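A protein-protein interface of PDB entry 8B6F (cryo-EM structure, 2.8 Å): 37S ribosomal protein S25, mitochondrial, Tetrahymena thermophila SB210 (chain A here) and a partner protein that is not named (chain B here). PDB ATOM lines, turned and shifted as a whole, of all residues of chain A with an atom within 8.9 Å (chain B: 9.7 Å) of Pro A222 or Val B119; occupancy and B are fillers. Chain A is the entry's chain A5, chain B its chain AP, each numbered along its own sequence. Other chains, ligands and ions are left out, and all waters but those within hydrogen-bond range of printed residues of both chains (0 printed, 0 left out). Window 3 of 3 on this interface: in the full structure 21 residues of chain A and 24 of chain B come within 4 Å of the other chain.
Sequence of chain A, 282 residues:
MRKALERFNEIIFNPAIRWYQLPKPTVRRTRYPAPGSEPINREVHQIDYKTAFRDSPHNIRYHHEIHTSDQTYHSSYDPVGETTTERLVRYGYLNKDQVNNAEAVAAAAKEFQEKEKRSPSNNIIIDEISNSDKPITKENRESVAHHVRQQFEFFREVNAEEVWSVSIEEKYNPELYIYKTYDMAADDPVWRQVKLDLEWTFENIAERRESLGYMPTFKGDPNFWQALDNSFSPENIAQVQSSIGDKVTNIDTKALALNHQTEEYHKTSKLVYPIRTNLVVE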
ATOM      1  N   LYS A 219       2.980  18.147  -7.596  1.00  0.00           N
ATOM      2  CA  LYS A 219       2.282  19.245  -8.251  1.00  0.00           C
ATOM      3  C   LYS A 219       1.933  20.310  -7.223  1.00  0.00           C
ATOM      4  O   LYS A 219       1.290  20.014  -6.212  1.00  0.00           O
ATOM      5  CB  LYS A 219       1.016  18.740  -8.948  1.00  0.00           C
ATOM      6  CG  LYS A 219       0.215  19.819  -9.674  1.00  0.00           C
ATOM      7  CD  LYS A 219       0.951  20.371 -10.885  1.00  0.00           C
ATOM      8  CE  LYS A 219       1.050  19.340 -12.000  1.00  0.00           C
ATOM      9  NZ  LYS A 219       1.643  19.911 -13.244  1.00  0.00           N
ATOM     10  N   GLY A 220       2.356  21.544  -7.484  1.00  0.00           N
ATOM     11  CA  GLY A 220       2.041  22.628  -6.570  1.00  0.00           C
ATOM     12  C   GLY A 220       0.544  22.866  -6.489  1.00  0.00           C
ATOM     13  O   GLY A 220      -0.171  22.789  -7.490  1.00  0.00           O
ATOM     14  N   ASP A 221       0.068  23.156  -5.284  1.00  0.00           N
ATOM     15  CA  ASP A 221      -1.356  23.373  -5.036  1.00  0.00           C
ATOM     16  C   ASP A 221      -1.530  24.655  -4.232  1.00  0.00           C
ATOM     17  O   ASP A 221      -1.123  24.699  -3.052  1.00  0.00           O
ATOM     18  CB  ASP A 221      -1.961  22.184  -4.297  1.00  0.00           C
ATOM     19  CG  ASP A 221      -3.473  22.172  -4.352  1.00  0.00           C
ATOM     20  OD1 ASP A 221      -4.055  23.105  -4.944  1.00  0.00           O
ATOM     21  OD2 ASP A 221      -4.083  21.232  -3.803  1.00  0.00           O
ATOM     22  N   PRO A 222      -2.118  25.710  -4.804  1.00  0.00           N
ATOM     23  CA  PRO A 222      -2.238  26.968  -4.048  1.00  0.00           C
ATOM     24  C   PRO A 222      -3.086  26.850  -2.797  1.00  0.00           C
ATOM     25  O   PRO A 222      -2.898  27.635  -1.860  1.00  0.00           O
ATOM     26  CB  PRO A 222      -2.862  27.931  -5.067  1.00  0.00           C
ATOM     27  CG  PRO A 222      -3.558  27.060  -6.036  1.00  0.00           C
ATOM     28  CD  PRO A 222      -2.729  25.818  -6.139  1.00  0.00           C
ATOM     29  N   ASN A 223      -4.022  25.900  -2.749  1.00  0.00           N
ATOM     30  CA  ASN A 223      -4.843  25.733  -1.556  1.00  0.00           C
ATOM     31  C   ASN A 223      -4.040  25.237  -0.363  1.00  0.00           C
ATOM     32  O   ASN A 223      -4.559  25.245   0.757  1.00  0.00           O
ATOM     33  CB  ASN A 223      -6.006  24.780  -1.846  1.00  0.00           C
ATOM     34  CG  ASN A 223      -5.549  23.398  -2.248  1.00  0.00           C
ATOM     35  OD1 ASN A 223      -4.494  22.930  -1.825  1.00  0.00           O
ATOM     36  ND2 ASN A 223      -6.346  22.733  -3.075  1.00  0.00           N
ATOM     37  N   PHE A 224      -2.799  24.798  -0.575  1.00  0.00           N
ATOM     38  CA  PHE A 224      -1.933  24.430   0.537  1.00  0.00           C
ATOM     39  C   PHE A 224      -1.657  25.609   1.462  1.00  0.00           C
ATOM     40  O   PHE A 224      -1.254  25.400   2.611  1.00  0.00           O
ATOM     41  CB  PHE A 224      -0.616  23.868  -0.002  1.00  0.00           C
ATOM     42  CG  PHE A 224       0.380  23.512   1.064  1.00  0.00           C
ATOM     43  CD1 PHE A 224       0.376  22.253   1.639  1.00  0.00           C
ATOM     44  CD2 PHE A 224       1.331  24.430   1.479  1.00  0.00           C
ATOM     45  CE1 PHE A 224       1.295  21.918   2.615  1.00  0.00           C
ATOM     46  CE2 PHE A 224       2.253  24.102   2.453  1.00  0.00           C
ATOM     47  CZ  PHE A 224       2.236  22.845   3.022  1.00  0.00           C
ATOM     48  N   TRP A 225      -1.864  26.839   0.989  1.00  0.00           N
ATOM     49  CA  TRP A 225      -1.570  28.044   1.754  1.00  0.00           C
ATOM     50  C   TRP A 225      -2.835  28.732   2.256  1.00  0.00           C
ATOM     51  O   TRP A 225      -2.888  29.961   2.330  1.00  0.00           O
ATOM     52  CB  TRP A 225      -0.743  29.015   0.914  1.00  0.00           C
ATOM     53  CG  TRP A 225       0.584  28.467   0.515  1.00  0.00           C
ATOM     54  CD1 TRP A 225       0.928  27.958  -0.701  1.00  0.00           C
ATOM     55  CD2 TRP A 225       1.750  28.366   1.338  1.00  0.00           C
ATOM     56  NE1 TRP A 225       2.237  27.548  -0.688  1.00  0.00           N
ATOM     57  CE2 TRP A 225       2.765  27.786   0.553  1.00  0.00           C
ATOM     58  CE3 TRP A 225       2.035  28.709   2.663  1.00  0.00           C
ATOM     59  CZ2 TRP A 225       4.044  27.545   1.047  1.00  0.00           C
ATOM     60  CZ3 TRP A 225       3.303  28.468   3.153  1.00  0.00           C
ATOM     61  CH2 TRP A 225       4.294  27.891   2.347  1.00  0.00           C
ATOM     62  N   GLN A 226      -3.860  27.961   2.603  1.00  0.00           N
ATOM     63  CA  GLN A 226      -5.055  28.543   3.189  1.00  0.00           C
ATOM     64  C   GLN A 226      -4.747  29.114   4.569  1.00  0.00           C
ATOM     65  O   GLN A 226      -3.824  28.675   5.258  1.00  0.00           O
ATOM     66  CB  GLN A 226      -6.166  27.500   3.295  1.00  0.00           C
ATOM     67  CG  GLN A 226      -6.857  27.200   1.978  1.00  0.00           C
ATOM     68  CD  GLN A 226      -8.024  26.244   2.135  1.00  0.00           C
ATOM     69  OE1 GLN A 226      -9.060  26.405   1.493  1.00  0.00           O
ATOM     70  NE2 GLN A 226      -7.859  25.236   2.987  1.00  0.00           N
ATOM     71  N   ALA A 227      -5.529  30.120   4.963  1.00  0.00           N
ATOM     72  CA  ALA A 227      -5.285  30.782   6.240  1.00  0.00           C
ATOM     73  C   ALA A 227      -5.471  29.822   7.409  1.00  0.00           C
ATOM     74  O   ALA A 227      -4.670  29.821   8.351  1.00  0.00           O
ATOM     75  CB  ALA A 227      -6.212  31.987   6.388  1.00  0.00           C
ATOM     76  N   GLN A 241     -11.337  32.823   4.476  1.00  0.00           N
ATOM     77  CA  GLN A 241     -10.923  32.956   3.085  1.00  0.00           C
ATOM     78  C   GLN A 241     -11.655  34.104   2.403  1.00  0.00           C
ATOM     79  O   GLN A 241     -11.049  34.886   1.663  1.00  0.00           O
ATOM     80  CB  GLN A 241     -11.161  31.642   2.344  1.00  0.00           C
ATOM     81  CG  GLN A 241     -10.295  30.496   2.848  1.00  0.00           C
ATOM     82  CD  GLN A 241      -8.820  30.718   2.578  1.00  0.00           C
ATOM     83  OE1 GLN A 241      -7.993  30.631   3.483  1.00  0.00           O
ATOM     84  NE2 GLN A 241      -8.484  30.999   1.325  1.00  0.00           N
ATOM     85  N   ILE A 244     -10.187  37.428   3.629  1.00  0.00           N
ATOM     86  CA  ILE A 244      -8.917  37.734   2.973  1.00  0.00           C
ATOM     87  C   ILE A 244      -9.052  37.798   1.462  1.00  0.00           C
ATOM     88  O   ILE A 244      -8.046  37.993   0.769  1.00  0.00           O
ATOM     89  CB  ILE A 244      -7.821  36.714   3.347  1.00  0.00           C
ATOM     90  CG1 ILE A 244      -8.134  35.338   2.751  1.00  0.00           C
ATOM     91  CG2 ILE A 244      -7.683  36.637   4.862  1.00  0.00           C
ATOM     92  CD1 ILE A 244      -7.116  34.260   3.085  1.00  0.00           C
ATOM     93  N   ASP A 246      -9.923  35.468  -0.946  1.00  0.00           N
ATOM     94  CA  ASP A 246      -9.388  34.360  -1.723  1.00  0.00           C
ATOM     95  C   ASP A 246     -10.473  33.811  -2.641  1.00  0.00           C
ATOM     96  O   ASP A 246     -11.558  33.445  -2.181  1.00  0.00           O
ATOM     97  CB  ASP A 246      -8.870  33.258  -0.801  1.00  0.00           C
ATOM     98  CG  ASP A 246      -8.259  32.099  -1.563  1.00  0.00           C
ATOM     99  OD1 ASP A 246      -8.110  32.207  -2.799  1.00  0.00           O
ATOM    100  OD2 ASP A 246      -7.930  31.076  -0.925  1.00  0.00           O
ATOM    101  N   LYS A 247     -10.172  33.758  -3.940  1.00  0.00           N
ATOM    102  CA  LYS A 247     -11.104  33.246  -4.934  1.00  0.00           C
ATOM    103  C   LYS A 247     -10.505  32.153  -5.810  1.00  0.00           C
ATOM    104  O   LYS A 247     -11.188  31.677  -6.724  1.00  0.00           O
ATOM    105  CB  LYS A 247     -11.612  34.387  -5.827  1.00  0.00           C
ATOM    106  CG  LYS A 247     -12.297  35.510  -5.063  1.00  0.00           C
ATOM    107  CD  LYS A 247     -12.743  36.622  -5.999  1.00  0.00           C
ATOM    108  CE  LYS A 247     -13.392  37.762  -5.232  1.00  0.00           C
ATOM    109  NZ  LYS A 247     -13.812  38.871  -6.135  1.00  0.00           N
ATOM    110  N   VAL A 248      -9.263  31.744  -5.563  1.00  0.00           N
ATOM    111  CA  VAL A 248      -8.596  30.708  -6.341  1.00  0.00           C
ATOM    112  C   VAL A 248      -8.449  29.418  -5.542  1.00  0.00           C
ATOM    113  O   VAL A 248      -7.699  28.523  -5.943  1.00  0.00           O
ATOM    114  CB  VAL A 248      -7.230  31.203  -6.856  1.00  0.00           C
ATOM    115  CG1 VAL A 248      -6.224  31.324  -5.715  1.00  0.00           C
ATOM    116  CG2 VAL A 248      -6.697  30.306  -7.977  1.00  0.00           C
ATOM    117  N   THR A 249      -9.156  29.296  -4.422  1.00  0.00           N
ATOM    118  CA  THR A 249      -9.089  28.120  -3.572  1.00  0.00           C
ATOM    119  C   THR A 249     -10.473  27.496  -3.461  1.00  0.00           C
ATOM    120  O   THR A 249     -11.492  28.180  -3.583  1.00  0.00           O
ATOM    121  CB  THR A 249      -8.558  28.482  -2.175  1.00  0.00           C
ATOM    122  OG1 THR A 249      -7.251  29.059  -2.291  1.00  0.00           O
ATOM    123  CG2 THR A 249      -8.485  27.260  -1.278  1.00  0.00           C
ATOM    124  N   ASN A 250     -10.499  26.185  -3.236  1.00  0.00           N
ATOM    125  CA  ASN A 250     -11.751  25.445  -3.108  1.00  0.00           C
ATOM    126  C   ASN A 250     -12.354  25.745  -1.742  1.00  0.00           C
ATOM    127  O   ASN A 250     -11.885  25.245  -0.718  1.00  0.00           O
ATOM    128  CB  ASN A 250     -11.505  23.953  -3.294  1.00  0.00           C
ATOM    129  CG  ASN A 250     -12.787  23.149  -3.305  1.00  0.00           C
ATOM    130  OD1 ASN A 250     -13.867  23.685  -3.547  1.00  0.00           O
ATOM    131  ND2 ASN A 250     -12.673  21.853  -3.042  1.00  0.00           N
ATOM    132  N   HIS A 266       0.353  15.344  -0.525  1.00  0.00           N
ATOM    133  CA  HIS A 266       0.210  16.511  -1.379  1.00  0.00           C
ATOM    134  C   HIS A 266      -0.233  16.098  -2.782  1.00  0.00           C
ATOM    135  O   HIS A 266      -0.182  14.928  -3.167  1.00  0.00           O
ATOM    136  CB  HIS A 266       1.529  17.282  -1.443  1.00  0.00           C
ATOM    137  CG  HIS A 266       1.377  18.707  -1.879  1.00  0.00           C
ATOM    138  ND1 HIS A 266       1.406  19.089  -3.203  1.00  0.00           N
ATOM    139  CD2 HIS A 266       1.205  19.842  -1.163  1.00  0.00           C
ATOM    140  CE1 HIS A 266       1.253  20.398  -3.284  1.00  0.00           C
ATOM    141  NE2 HIS A 266       1.128  20.880  -2.061  1.00  0.00           N
ATOM    142  N   LYS A 267      -0.677  17.092  -3.548  1.00  0.00           N
ATOM    143  CA  LYS A 267      -1.173  16.845  -4.895  1.00  0.00           C
ATOM    144  C   LYS A 267      -0.062  16.294  -5.779  1.00  0.00           C
ATOM    145  O   LYS A 267       1.080  16.759  -5.737  1.00  0.00           O
ATOM    146  CB  LYS A 267      -1.728  18.139  -5.490  1.00  0.00           C
ATOM    147  CG  LYS A 267      -2.393  17.968  -6.844  1.00  0.00           C
ATOM    148  CD  LYS A 267      -2.916  19.295  -7.365  1.00  0.00           C
ATOM    149  CE  LYS A 267      -3.577  19.132  -8.724  1.00  0.00           C
ATOM    150  NZ  LYS A 267      -4.095  20.428  -9.250  1.00  0.00           N
ATOM    151  N   VAL B  96       8.086  36.526 -11.886  1.00  0.00           N
ATOM    152  CA  VAL B  96       8.390  35.609 -10.791  1.00  0.00           C
ATOM    153  C   VAL B  96       7.910  34.199 -11.115  1.00  0.00           C
ATOM    154  O   VAL B  96       8.602  33.214 -10.832  1.00  0.00           O
ATOM    155  CB  VAL B  96       7.780  36.135  -9.479  1.00  0.00           C
ATOM    156  CG1 VAL B  96       8.277  37.546  -9.206  1.00  0.00           C
ATOM    157  CG2 VAL B  96       6.259  36.101  -9.523  1.00  0.00           C
ATOM    158  N   GLY B  97       6.719  34.075 -11.701  1.00  0.00           N
ATOM    159  CA  GLY B  97       6.187  32.753 -11.988  1.00  0.00           C
ATOM    160  C   GLY B  97       7.032  31.980 -12.980  1.00  0.00           C
ATOM    161  O   GLY B  97       7.306  30.793 -12.784  1.00  0.00           O
ATOM    162  N   TYR B 106      11.183  23.855 -11.183  1.00  0.00           N
ATOM    163  CA  TYR B 106      10.010  22.997 -11.213  1.00  0.00           C
ATOM    164  C   TYR B 106       9.445  23.015 -12.623  1.00  0.00           C
ATOM    165  O   TYR B 106       9.731  23.916 -13.414  1.00  0.00           O
ATOM    166  CB  TYR B 106       8.950  23.451 -10.206  1.00  0.00           C
ATOM    167  CG  TYR B 106       8.749  24.942 -10.191  1.00  0.00           C
ATOM    168  CD1 TYR B 106       8.021  25.563 -11.193  1.00  0.00           C
ATOM    169  CD2 TYR B 106       9.281  25.729  -9.179  1.00  0.00           C
ATOM    170  CE1 TYR B 106       7.829  26.918 -11.197  1.00  0.00           C
ATOM    171  CE2 TYR B 106       9.093  27.098  -9.174  1.00  0.00           C
ATOM    172  CZ  TYR B 106       8.361  27.684 -10.191  1.00  0.00           C
ATOM    173  OH  TYR B 106       8.146  29.038 -10.226  1.00  0.00           O
ATOM    174  N   ASP B 108       6.201  23.172 -13.336  1.00  0.00           N
ATOM    175  CA  ASP B 108       4.934  23.888 -13.385  1.00  0.00           C
ATOM    176  C   ASP B 108       5.161  25.315 -13.863  1.00  0.00           C
ATOM    177  O   ASP B 108       6.176  25.935 -13.539  1.00  0.00           O
ATOM    178  CB  ASP B 108       4.269  23.904 -12.009  1.00  0.00           C
ATOM    179  CG  ASP B 108       4.047  22.515 -11.454  1.00  0.00           C
ATOM    180  OD1 ASP B 108       4.277  21.535 -12.192  1.00  0.00           O
ATOM    181  OD2 ASP B 108       3.652  22.402 -10.275  1.00  0.00           O
ATOM    182  N   PRO B 110       3.064  29.257 -14.731  1.00  0.00           N
ATOM    183  CA  PRO B 110       1.838  30.022 -14.480  1.00  0.00           C
ATOM    184  C   PRO B 110       0.827  29.832 -15.597  1.00  0.00           C
ATOM    185  O   PRO B 110       1.176  29.775 -16.778  1.00  0.00           O
ATOM    186  CB  PRO B 110       2.331  31.471 -14.409  1.00  0.00           C
ATOM    187  CG  PRO B 110       3.765  31.370 -14.061  1.00  0.00           C
ATOM    188  CD  PRO B 110       4.259  30.119 -14.715  1.00  0.00           C
ATOM    189  N   THR B 111      -0.442  29.735 -15.210  1.00  0.00           N
ATOM    190  CA  THR B 111      -1.546  29.609 -16.152  1.00  0.00           C
ATOM    191  C   THR B 111      -2.571  30.677 -15.822  1.00  0.00           C
ATOM    192  O   THR B 111      -3.089  30.714 -14.701  1.00  0.00           O
ATOM    193  CB  THR B 111      -2.185  28.218 -16.085  1.00  0.00           C
ATOM    194  OG1 THR B 111      -2.733  28.003 -14.778  1.00  0.00           O
ATOM    195  CG2 THR B 111      -1.156  27.141 -16.383  1.00  0.00           C
ATOM    196  N   GLY B 114      -7.209  29.690 -14.845  1.00  0.00           N
ATOM    197  CA  GLY B 114      -7.304  28.248 -14.729  1.00  0.00           C
ATOM    198  C   GLY B 114      -6.684  27.795 -13.429  1.00  0.00           C
ATOM    199  O   GLY B 114      -6.145  28.594 -12.655  1.00  0.00           O
ATOM    200  N   ASN B 115      -6.767  26.487 -13.194  1.00  0.00           N
ATOM    201  CA  ASN B 115      -6.156  25.903 -12.009  1.00  0.00           C
ATOM    202  C   ASN B 115      -4.650  26.109 -12.053  1.00  0.00           C
ATOM    203  O   ASN B 115      -3.958  25.509 -12.882  1.00  0.00           O
ATOM    204  CB  ASN B 115      -6.490  24.414 -11.905  1.00  0.00           C
ATOM    205  CG  ASN B 115      -7.969  24.163 -11.705  1.00  0.00           C
ATOM    206  OD1 ASN B 115      -8.801  25.021 -11.997  1.00  0.00           O
ATOM    207  ND2 ASN B 115      -8.305  22.980 -11.204  1.00  0.00           N
ATOM    208  N   SER B 116      -4.138  26.956 -11.169  1.00  0.00           N
ATOM    209  CA  SER B 116      -2.728  27.312 -11.149  1.00  0.00           C
ATOM    210  C   SER B 116      -2.010  26.578 -10.026  1.00  0.00           C
ATOM    211  O   SER B 116      -2.617  26.135  -9.050  1.00  0.00           O
ATOM    212  CB  SER B 116      -2.557  28.824 -10.976  1.00  0.00           C
ATOM    213  OG  SER B 116      -3.142  29.264  -9.763  1.00  0.00           O
ATOM    214  N   ALA B 117      -0.697  26.447 -10.187  1.00  0.00           N
ATOM    215  CA  ALA B 117       0.162  25.861  -9.171  1.00  0.00           C
ATOM    216  C   ALA B 117       0.796  26.904  -8.263  1.00  0.00           C
ATOM    217  O   ALA B 117       1.600  26.542  -7.399  1.00  0.00           O
ATOM    218  CB  ALA B 117       1.260  25.025  -9.834  1.00  0.00           C
ATOM    219  N   PHE B 118       0.457  28.178  -8.437  1.00  0.00           N
ATOM    220  CA  PHE B 118       1.048  29.266  -7.673  1.00  0.00           C
ATOM    221  C   PHE B 118      -0.047  30.036  -6.954  1.00  0.00           C
ATOM    222  O   PHE B 118      -1.118  30.284  -7.517  1.00  0.00           O
ATOM    223  CB  PHE B 118       1.839  30.206  -8.585  1.00  0.00           C
ATOM    224  CG  PHE B 118       2.861  29.505  -9.426  1.00  0.00           C
ATOM    225  CD1 PHE B 118       2.516  28.969 -10.655  1.00  0.00           C
ATOM    226  CD2 PHE B 118       4.168  29.375  -8.986  1.00  0.00           C
ATOM    227  CE1 PHE B 118       3.453  28.321 -11.430  1.00  0.00           C
ATOM    228  CE2 PHE B 118       5.108  28.727  -9.756  1.00  0.00           C
ATOM    229  CZ  PHE B 118       4.750  28.199 -10.981  1.00  0.00           C
ATOM    230  N   VAL B 119       0.229  30.415  -5.707  1.00  0.00           N
ATOM    231  CA  VAL B 119      -0.765  31.105  -4.896  1.00  0.00           C
ATOM    232  C   VAL B 119      -0.909  32.543  -5.370  1.00  0.00           C
ATOM    233  O   VAL B 119       0.065  33.182  -5.789  1.00  0.00           O
ATOM    234  CB  VAL B 119      -0.373  31.037  -3.411  1.00  0.00           C
ATOM    235  CG1 VAL B 119       0.869  31.879  -3.134  1.00  0.00           C
ATOM    236  CG2 VAL B 119      -1.538  31.471  -2.541  1.00  0.00           C
ATOM    237  N   LYS B 120      -2.134  33.060  -5.307  1.00  0.00           N
ATOM    238  CA  LYS B 120      -2.457  34.419  -5.732  1.00  0.00           C
ATOM    239  C   LYS B 120      -3.101  35.139  -4.551  1.00  0.00           C
ATOM    240  O   LYS B 120      -4.327  35.156  -4.412  1.00  0.00           O
ATOM    241  CB  LYS B 120      -3.378  34.402  -6.949  1.00  0.00           C
ATOM    242  CG  LYS B 120      -2.798  33.675  -8.150  1.00  0.00           C
ATOM    243  CD  LYS B 120      -3.816  33.570  -9.271  1.00  0.00           C
ATOM    244  CE  LYS B 120      -3.211  32.936 -10.513  1.00  0.00           C
ATOM    245  NZ  LYS B 120      -4.210  32.799 -11.610  1.00  0.00           N
ATOM    246  N   HIS B 121      -2.271  35.739  -3.704  1.00  0.00           N
ATOM    247  CA  HIS B 121      -2.764  36.454  -2.539  1.00  0.00           C
ATOM    248  C   HIS B 121      -3.207  37.863  -2.922  1.00  0.00           C
ATOM    249  O   HIS B 121      -2.886  38.377  -3.997  1.00  0.00           O
ATOM    250  CB  HIS B 121      -1.694  36.524  -1.451  1.00  0.00           C
ATOM    251  CG  HIS B 121      -1.294  35.189  -0.908  1.00  0.00           C
ATOM    252  ND1 HIS B 121      -2.144  34.410  -0.151  1.00  0.00           N
ATOM    253  CD2 HIS B 121      -0.136  34.497  -1.003  1.00  0.00           C
ATOM    254  CE1 HIS B 121      -1.525  33.297   0.195  1.00  0.00           C
ATOM    255  NE2 HIS B 121      -0.305  33.323  -0.309  1.00  0.00           N
ATOM    256  N   HIS B 122      -3.957  38.489  -2.015  1.00  0.00           N
ATOM    257  CA  HIS B 122      -4.498  39.815  -2.284  1.00  0.00           C
ATOM    258  C   HIS B 122      -3.440  40.907  -2.190  1.00  0.00           C
ATOM    259  O   HIS B 122      -3.619  41.973  -2.788  1.00  0.00           O
ATOM    260  CB  HIS B 122      -5.640  40.119  -1.314  1.00  0.00           C
ATOM    261  CG  HIS B 122      -5.208  40.220   0.115  1.00  0.00           C
ATOM    262  ND1 HIS B 122      -4.933  39.114   0.892  1.00  0.00           N
ATOM    263  CD2 HIS B 122      -5.010  41.296   0.912  1.00  0.00           C
ATOM    264  CE1 HIS B 122      -4.581  39.506   2.104  1.00  0.00           C
ATOM    265  NE2 HIS B 122      -4.619  40.824   2.143  1.00  0.00           N
ATOM    266  N   TYR B 123      -2.354  40.673  -1.461  1.00  0.00           N
ATOM    267  CA  TYR B 123      -1.333  41.689  -1.246  1.00  0.00           C
ATOM    268  C   TYR B 123      -0.191  41.620  -2.250  1.00  0.00           C
ATOM    269  O   TYR B 123       0.757  42.403  -2.137  1.00  0.00           O
ATOM    270  CB  TYR B 123      -0.768  41.573   0.175  1.00  0.00           C
ATOM    271  CG  TYR B 123      -0.076  40.260   0.460  1.00  0.00           C
ATOM    272  CD1 TYR B 123       1.263  40.074   0.143  1.00  0.00           C
ATOM    273  CD2 TYR B 123      -0.758  39.210   1.058  1.00  0.00           C
ATOM    274  CE1 TYR B 123       1.900  38.877   0.405  1.00  0.00           C
ATOM    275  CE2 TYR B 123      -0.132  38.009   1.324  1.00  0.00           C
ATOM    276  CZ  TYR B 123       1.198  37.849   0.996  1.00  0.00           C
ATOM    277  OH  TYR B 123       1.826  36.655   1.259  1.00  0.00           O
ATOM    278  N   LEU B 124      -0.251  40.716  -3.221  1.00  0.00           N
ATOM    279  CA  LEU B 124       0.841  40.573  -4.173  1.00  0.00           C
ATOM    280  C   LEU B 124       0.950  41.803  -5.067  1.00  0.00           C
ATOM    281  O   LEU B 124      -0.030  42.508  -5.318  1.00  0.00           O
ATOM    282  CB  LEU B 124       0.642  39.323  -5.030  1.00  0.00           C
ATOM    283  CG  LEU B 124       0.566  37.989  -4.282  1.00  0.00           C
ATOM    284  CD1 LEU B 124       0.450  36.843  -5.269  1.00  0.00           C
ATOM    285  CD2 LEU B 124       1.767  37.787  -3.371  1.00  0.00           C
ATOM    286  N   LYS B 125       2.165  42.054  -5.548  1.00  0.00           N
ATOM    287  CA  LYS B 125       2.457  43.168  -6.437  1.00  0.00           C
ATOM    288  C   LYS B 125       3.030  42.644  -7.747  1.00  0.00           C
ATOM    289  O   LYS B 125       3.620  41.560  -7.796  1.00  0.00           O
ATOM    290  CB  LYS B 125       3.448  44.148  -5.797  1.00  0.00           C
ATOM    291  CG  LYS B 125       2.922  44.839  -4.551  1.00  0.00           C
ATOM    292  CD  LYS B 125       3.949  45.811  -3.990  1.00  0.00           C
ATOM    293  CE  LYS B 125       3.403  46.552  -2.780  1.00  0.00           C
ATOM    294  NZ  LYS B 125       4.405  47.493  -2.204  1.00  0.00           N
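OG of Ser B116 lies within hydrogen-bond range of O of Phe B118, 3.2 Å away. ND1 of His A266 lies close to O of Lys A219. The backbone NH (N) of Lys A219 lies within hydrogen-bond range of the backbone carbonyl oxygen (O) of Lys A267, at 3.0 Å.
Ala B117 touches Gly A220. Pro A222 touches Ser B116 (CD to O, 2.9 Å). CB of Pro A222 touches O of Phe B118 (3.8 Å). Pro A222 touches Val B119 (CB to CA, 3.8 Å).
Of the 18 printed residues of chain B, 6 touch a printed residue of chain A. Printed residues of chain B that touch a printed residue of chain A: Asp B108, Ser B116, Ala B117, Phe B118, Val B119 and His B122. Among the printed residues, 7 pairs touch across the chains. Among the printed residues, Asp or Glu carboxylates within 4 Å of a Lys or Arg side-chain nitrogen of the other chain: Lys A219 with Asp B108 (3.3 Å).
The side-chain carboxylate of Asp B108 is in salt-bridge range of the side-chain amino group of Lys A219, 3.3 Å away. The side-chain carboxylate (OD2) of Asp B108 sits at hydrogen-bond distance from the backbone NH (N) of Gly A220. ND1 of His B122 is in hydrogen-bond range of O of Ile A244 (3.3 Å).
Of chain B, only Ser B116 (2.9 Å), Phe B118 (3.8 Å) and Val B119 (3.8 Å) come within 4 Å of Pro A222. Val B119 touches one residue of chain A. No residue of chain B comes within 4 Å of Asp A221. Of the printed residues of chain A, Ser B116 touches Pro A222. Printed residues of chain A within 4 Å of Ala B117: Gly A220 (3.5 Å). Printed residues of chain B within 4 Å of Ile A244: His B122 (3.3 Å). Asn A250 touches none of the printed residues of chain B. Pro B110 touches none of the printed residues of chain A. The nearest residue of chain B that does not touch Pro A222 is Ala B117 (4.2 Å). The nearest residue of chain A that does not touch Val B119 is Trp A225 (4.3 Å). The nearest printed residue of chain B that does not touch Ile A244 is His B121 (5.9 Å).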
